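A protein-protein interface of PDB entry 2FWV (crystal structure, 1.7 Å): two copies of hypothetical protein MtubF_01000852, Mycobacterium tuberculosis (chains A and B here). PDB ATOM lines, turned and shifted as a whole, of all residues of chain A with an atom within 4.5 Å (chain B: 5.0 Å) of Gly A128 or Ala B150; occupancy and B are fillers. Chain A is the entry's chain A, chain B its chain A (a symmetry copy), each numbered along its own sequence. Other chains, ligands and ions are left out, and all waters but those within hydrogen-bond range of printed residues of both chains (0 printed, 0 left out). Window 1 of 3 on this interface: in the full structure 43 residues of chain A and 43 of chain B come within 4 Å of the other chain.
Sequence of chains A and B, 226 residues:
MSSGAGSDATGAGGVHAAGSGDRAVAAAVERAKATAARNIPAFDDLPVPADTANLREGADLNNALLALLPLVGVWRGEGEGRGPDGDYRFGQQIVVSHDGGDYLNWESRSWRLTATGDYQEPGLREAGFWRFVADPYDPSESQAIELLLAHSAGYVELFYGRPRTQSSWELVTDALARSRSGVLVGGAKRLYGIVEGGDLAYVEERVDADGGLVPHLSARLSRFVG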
ATOM      1  N   LEU A 104       2.742   5.179   3.481  1.00  0.00           N
ATOM      2  CA  LEU A 104       4.141   5.523   3.790  1.00  0.00           C
ATOM      3  C   LEU A 104       4.211   6.037   5.234  1.00  0.00           C
ATOM      4  O   LEU A 104       3.314   6.773   5.667  1.00  0.00           O
ATOM      5  CB  LEU A 104       4.658   6.627   2.890  1.00  0.00           C
ATOM      6  CG  LEU A 104       4.584   6.319   1.386  1.00  0.00           C
ATOM      7  CD1 LEU A 104       5.095   7.544   0.648  1.00  0.00           C
ATOM      8  CD2 LEU A 104       5.470   5.114   1.068  1.00  0.00           C
ATOM      9  N   ASN A 105       5.234   5.612   5.952  1.00  0.00           N
ATOM     10  CA  ASN A 105       5.559   6.229   7.244  1.00  0.00           C
ATOM     11  C   ASN A 105       6.179   7.590   6.998  1.00  0.00           C
ATOM     12  O   ASN A 105       7.082   7.710   6.162  1.00  0.00           O
ATOM     13  CB  ASN A 105       6.587   5.369   7.981  1.00  0.00           C
ATOM     14  CG  ASN A 105       6.192   3.922   8.093  1.00  0.00           C
ATOM     15  OD1 ASN A 105       6.998   3.025   7.788  1.00  0.00           O
ATOM     16  ND2 ASN A 105       4.985   3.671   8.492  1.00  0.00           N
ATOM     17  N   TRP A 106       5.794   8.604   7.804  1.00  0.00           N
ATOM     18  CA  TRP A 106       6.338   9.954   7.635  1.00  0.00           C
ATOM     19  C   TRP A 106       6.802  10.493   8.997  1.00  0.00           C
ATOM     20  O   TRP A 106       6.075  10.384   9.972  1.00  0.00           O
ATOM     21  CB  TRP A 106       5.192  10.820   7.150  1.00  0.00           C
ATOM     22  CG  TRP A 106       5.427  12.300   7.098  1.00  0.00           C
ATOM     23  CD1 TRP A 106       5.109  13.251   8.066  1.00  0.00           C
ATOM     24  CD2 TRP A 106       5.976  13.008   5.986  1.00  0.00           C
ATOM     25  NE1 TRP A 106       5.434  14.517   7.585  1.00  0.00           N
ATOM     26  CE2 TRP A 106       5.962  14.393   6.322  1.00  0.00           C
ATOM     27  CE3 TRP A 106       6.433  12.611   4.699  1.00  0.00           C
ATOM     28  CZ2 TRP A 106       6.411  15.384   5.431  1.00  0.00           C
ATOM     29  CZ3 TRP A 106       6.898  13.612   3.806  1.00  0.00           C
ATOM     30  CH2 TRP A 106       6.870  14.991   4.188  1.00  0.00           C
ATOM     31  N   ALA A 127       4.593  13.302  12.965  1.00  0.00           N
ATOM     32  CA  ALA A 127       4.690  11.932  12.562  1.00  0.00           C
ATOM     33  C   ALA A 127       3.359  11.490  12.069  1.00  0.00           C
ATOM     34  O   ALA A 127       2.308  11.907  12.587  1.00  0.00           O
ATOM     35  CB  ALA A 127       5.106  11.060  13.720  1.00  0.00           C
ATOM     36  N   GLY A 128       3.391  10.598  11.085  1.00  0.00           N
ATOM     37  CA  GLY A 128       2.129  10.024  10.638  1.00  0.00           C
ATOM     38  C   GLY A 128       2.294   9.207   9.375  1.00  0.00           C
ATOM     39  O   GLY A 128       3.305   8.498   9.249  1.00  0.00           O
ATOM     40  N   PHE A 129       1.294   9.299   8.495  1.00  0.00           N
ATOM     41  CA  PHE A 129       1.191   8.372   7.343  1.00  0.00           C
ATOM     42  C   PHE A 129       0.627   9.070   6.121  1.00  0.00           C
ATOM     43  O   PHE A 129      -0.273   9.918   6.233  1.00  0.00           O
ATOM     44  CB  PHE A 129       0.300   7.153   7.688  1.00  0.00           C
ATOM     45  CG  PHE A 129       0.754   6.416   8.890  1.00  0.00           C
ATOM     46  CD1 PHE A 129       1.788   5.515   8.810  1.00  0.00           C
ATOM     47  CD2 PHE A 129       0.167   6.685  10.123  1.00  0.00           C
ATOM     48  CE1 PHE A 129       2.279   4.875   9.945  1.00  0.00           C
ATOM     49  CE2 PHE A 129       0.626   6.028  11.282  1.00  0.00           C
ATOM     50  CZ  PHE A 129       1.675   5.121  11.173  1.00  0.00           C
ATOM     51  N   LEU A 148      -1.984  11.965   7.277  1.00  0.00           N
ATOM     52  CA  LEU A 148      -2.537  11.907   8.627  1.00  0.00           C
ATOM     53  C   LEU A 148      -1.380  12.194   9.579  1.00  0.00           C
ATOM     54  O   LEU A 148      -0.369  11.505   9.529  1.00  0.00           O
ATOM     55  CB  LEU A 148      -3.117  10.510   8.891  1.00  0.00           C
ATOM     56  CG  LEU A 148      -4.214  10.253   7.861  1.00  0.00           C
ATOM     57  CD1 LEU A 148      -3.707   9.218   6.808  1.00  0.00           C
ATOM     58  CD2 LEU A 148      -5.475   9.832   8.481  1.00  0.00           C
ATOM     59  N   LEU A 149      -1.516  13.210  10.426  1.00  0.00           N
ATOM     60  CA  LEU A 149      -0.366  13.658  11.241  1.00  0.00           C
ATOM     61  C   LEU A 149      -0.725  13.838  12.720  1.00  0.00           C
ATOM     62  O   LEU A 149      -1.811  14.310  13.064  1.00  0.00           O
ATOM     63  CB  LEU A 149       0.161  15.036  10.768  1.00  0.00           C
ATOM     64  CG  LEU A 149       0.809  15.123   9.380  1.00  0.00           C
ATOM     65  CD1 LEU A 149       1.207  16.599   9.142  1.00  0.00           C
ATOM     66  CD2 LEU A 149       2.046  14.250   9.337  1.00  0.00           C
ATOM     67  N   ALA A 150       0.236  13.479  13.570  1.00  0.00           N
ATOM     68  CA  ALA A 150       0.248  13.961  14.949  1.00  0.00           C
ATOM     69  C   ALA A 150       1.402  14.955  15.026  1.00  0.00           C
ATOM     70  O   ALA A 150       2.466  14.743  14.408  1.00  0.00           O
ATOM     71  CB  ALA A 150       0.509  12.789  15.910  1.00  0.00           C
ATOM     72  N   ARG B 125      -0.792  -0.057  12.568  1.00  0.00           N
ATOM     73  CA  ARG B 125       0.333   0.777  13.051  1.00  0.00           C
ATOM     74  C   ARG B 125      -0.175   2.150  13.468  1.00  0.00           C
ATOM     75  O   ARG B 125      -1.068   2.691  12.849  1.00  0.00           O
ATOM     76  CB  ARG B 125       1.348   0.933  11.879  1.00  0.00           C
ATOM     77  CG  ARG B 125       2.613   1.633  12.231  1.00  0.00           C
ATOM     78  CD  ARG B 125       3.676   1.374  11.151  1.00  0.00           C
ATOM     79  NE  ARG B 125       4.888   2.112  11.451  1.00  0.00           N
ATOM     80  CZ  ARG B 125       6.090   1.745  11.007  1.00  0.00           C
ATOM     81  NH1 ARG B 125       6.198   0.707  10.174  1.00  0.00           N
ATOM     82  NH2 ARG B 125       7.158   2.464  11.331  1.00  0.00           N
ATOM     83  N   GLU B 126       0.406   2.730  14.516  1.00  0.00           N
ATOM     84  CA  GLU B 126       0.036   4.106  14.902  1.00  0.00           C
ATOM     85  C   GLU B 126       1.307   4.822  15.332  1.00  0.00           C
ATOM     86  O   GLU B 126       2.281   4.196  15.726  1.00  0.00           O
ATOM     87  CB  GLU B 126      -0.994   4.117  16.044  1.00  0.00           C
ATOM     88  CG  GLU B 126      -0.492   3.414  17.296  1.00  0.00           C
ATOM     89  CD  GLU B 126      -1.568   3.297  18.408  1.00  0.00           C
ATOM     90  OE1 GLU B 126      -2.721   2.870  18.109  1.00  0.00           O
ATOM     91  OE2 GLU B 126      -1.247   3.628  19.578  1.00  0.00           O
ATOM     92  N   ALA B 127       1.298   6.145  15.232  1.00  0.00           N
ATOM     93  CA  ALA B 127       2.431   6.938  15.601  1.00  0.00           C
ATOM     94  C   ALA B 127       1.944   8.233  16.144  1.00  0.00           C
ATOM     95  O   ALA B 127       0.929   8.785  15.684  1.00  0.00           O
ATOM     96  CB  ALA B 127       3.314   7.200  14.406  1.00  0.00           C
ATOM     97  N   GLY B 128       2.695   8.758  17.106  1.00  0.00           N
ATOM     98  CA  GLY B 128       2.352  10.085  17.598  1.00  0.00           C
ATOM     99  C   GLY B 128       3.143  10.453  18.834  1.00  0.00           C
ATOM    100  O   GLY B 128       4.338  10.127  18.899  1.00  0.00           O
ATOM    101  N   LEU B 148      -1.610  11.933  21.184  1.00  0.00           N
ATOM    102  CA  LEU B 148      -1.981  12.425  19.861  1.00  0.00           C
ATOM    103  C   LEU B 148      -1.507  11.372  18.863  1.00  0.00           C
ATOM    104  O   LEU B 148      -0.330  11.035  18.851  1.00  0.00           O
ATOM    105  CB  LEU B 148      -1.289  13.769  19.593  1.00  0.00           C
ATOM    106  CG  LEU B 148      -1.745  14.755  20.666  1.00  0.00           C
ATOM    107  CD1 LEU B 148      -0.578  15.004  21.673  1.00  0.00           C
ATOM    108  CD2 LEU B 148      -2.254  16.007  20.096  1.00  0.00           C
ATOM    109  N   LEU B 149      -2.413  10.845  18.045  1.00  0.00           N
ATOM    110  CA  LEU B 149      -2.061   9.692  17.188  1.00  0.00           C
ATOM    111  C   LEU B 149      -2.496   9.884  15.731  1.00  0.00           C
ATOM    112  O   LEU B 149      -3.568  10.425  15.447  1.00  0.00           O
ATOM    113  CB  LEU B 149      -2.762   8.396  17.665  1.00  0.00           C
ATOM    114  CG  LEU B 149      -2.352   7.813  19.024  1.00  0.00           C
ATOM    115  CD1 LEU B 149      -3.222   6.558  19.276  1.00  0.00           C
ATOM    116  CD2 LEU B 149      -0.890   7.419  18.992  1.00  0.00           C
ATOM    117  N   ALA B 150      -1.646   9.394  14.830  1.00  0.00           N
ATOM    118  CA  ALA B 150      -2.072   9.106  13.463  1.00  0.00           C
ATOM    119  C   ALA B 150      -2.103   7.585  13.355  1.00  0.00           C
ATOM    120  O   ALA B 150      -1.232   6.890  13.918  1.00  0.00           O
ATOM    121  CB  ALA B 150      -1.048   9.675  12.466  1.00  0.00           C
ATOM    122  N   HIS B 151      -3.057   7.072  12.567  1.00  0.00           N
ATOM    123  CA  HIS B 151      -3.196   5.640  12.414  1.00  0.00           C
ATOM    124  C   HIS B 151      -3.031   5.268  10.944  1.00  0.00           C
ATOM    125  O   HIS B 151      -3.654   5.911  10.104  1.00  0.00           O
ATOM    126  CB  HIS B 151      -4.596   5.190  12.822  1.00  0.00           C
ATOM    127  CG  HIS B 151      -4.891   5.338  14.294  1.00  0.00           C
ATOM    128  ND1 HIS B 151      -4.666   4.320  15.199  1.00  0.00           N
ATOM    129  CD2 HIS B 151      -5.446   6.356  14.988  1.00  0.00           C
ATOM    130  CE1 HIS B 151      -5.059   4.719  16.407  1.00  0.00           C
ATOM    131  NE2 HIS B 151      -5.544   5.945  16.299  1.00  0.00           N
ATOM    132  N   SER B 152      -2.259   4.219  10.679  1.00  0.00           N
ATOM    133  CA  SER B 152      -1.991   3.798   9.261  1.00  0.00           C
ATOM    134  C   SER B 152      -3.275   3.431   8.537  1.00  0.00           C
ATOM    135  O   SER B 152      -3.334   3.527   7.277  1.00  0.00           O
ATOM    136  CB  SER B 152      -0.983   2.629   9.254  1.00  0.00           C
ATOM    137  OG  SER B 152      -1.518   1.486   9.917  1.00  0.00           O
ATOM    138  N   TYR B 155      -6.922   7.257   9.984  1.00  0.00           N
ATOM    139  CA  TYR B 155      -7.595   8.293  10.787  1.00  0.00           C
ATOM    140  C   TYR B 155      -6.617   8.877  11.802  1.00  0.00           C
ATOM    141  O   TYR B 155      -5.557   8.282  12.025  1.00  0.00           O
ATOM    142  CB  TYR B 155      -8.862   7.739  11.442  1.00  0.00           C
ATOM    143  CG  TYR B 155      -8.676   6.618  12.462  1.00  0.00           C
ATOM    144  CD1 TYR B 155      -8.454   5.289  12.051  1.00  0.00           C
ATOM    145  CD2 TYR B 155      -8.763   6.871  13.848  1.00  0.00           C
ATOM    146  CE1 TYR B 155      -8.291   4.246  12.982  1.00  0.00           C
ATOM    147  CE2 TYR B 155      -8.633   5.819  14.794  1.00  0.00           C
ATOM    148  CZ  TYR B 155      -8.390   4.509  14.338  1.00  0.00           C
ATOM    149  OH  TYR B 155      -8.244   3.458  15.201  1.00  0.00           O
ATOM    150  N   VAL B 156      -6.977  10.043  12.336  1.00  0.00           N
ATOM    151  CA  VAL B 156      -6.222  10.632  13.475  1.00  0.00           C
ATOM    152  C   VAL B 156      -7.128  10.589  14.717  1.00  0.00           C
ATOM    153  O   VAL B 156      -8.351  10.530  14.619  1.00  0.00           O
ATOM    154  CB  VAL B 156      -5.739  12.066  13.204  1.00  0.00           C
ATOM    155  CG1 VAL B 156      -4.682  12.081  12.040  1.00  0.00           C
ATOM    156  CG2 VAL B 156      -6.923  12.998  12.857  1.00  0.00           C
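ND2 of Asn A105 lies close to NE of Arg B125.
The backbone NH (N) of Trp A106 lies within hydrogen-bond range of the backbone carbonyl oxygen (O) of Gly A128 (2.9 Å). N of Ala A150 lies within hydrogen-bond range of O of Ala A127, 2.8 Å away. O of Phe A129 sits at hydrogen-bond distance from N of Leu A148 (2.9 Å). N of Ser B152 is in hydrogen-bond range of O of Arg B125. N of Ala B150 lies within hydrogen-bond range of O of Ala B127, 2.8 Å away.
Gly A128 touches Ala B150 (CA to CB, 3.7 Å). Phe A129 touches Arg B125. CE2 of Phe A129 touches O of Ala B150, at 3.3 Å. Phe A129 touches His B151. N of Ser B152 touches CE2 of Phe A129 (3.5 Å). Leu A148 touches Ala B150 (O to CB, 3.5 Å). N of Tyr B155 touches CD2 of Leu A148 (3.3 Å). Leu A148 touches Val B156 (CB to CG1, 3.9 Å). Leu A149 touches Val B156 (N to CG1, 3.7 Å). O of Leu B148 touches CB of Ala A150 (3.5 Å).
Trp A106 touches none of the printed residues of chain B. Of chain B, only Ala B150 comes within 4 Å of Gly A128. Printed residues of chain B within 4 Å of Phe A129: Arg B125 (3.8 Å), Ala B150 (3.3 Å), His B151 (3.6 Å) and Ser B152 (3.5 Å). Of the printed residues of chain B, Leu A149 touches Val B156. Of the printed residues of chain B, Ala A150 touches Gly B128 (3.7 Å) and Leu B148 (3.5 Å). Glu B126 touches none of the printed residues of chain A. Printed residues of chain A within 4 Å of Tyr B155: Leu A148. Of the printed residues of chain A, Val B156 touches Leu A148 and Leu A149. The nearest printed residue of chain A that does not touch Tyr B155 is Phe A129 (6.2 Å).
Along chain A the printed residues that touch a printed residue of chain B span positions 105 to 150. Printed residues of chain B that touch a printed residue of chain A: Arg B125, Gly B128, Leu B148, Ala B150, His B151, Ser B152, Tyr B155 and Val B156. Hydrophobic or aromatic side chains of chain B that line the printed part of chain A: Ala B150 and Val B156. Among the printed residues, 12 pairs touch across the chains.
Gly A128 touches Ala B150, and with the chains exchanged Ala A150 touches Gly B128. Leu A148 touches Ala B150, and with the chains exchanged Ala A150 touches Leu B148. 5 positions are printed for both chains.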
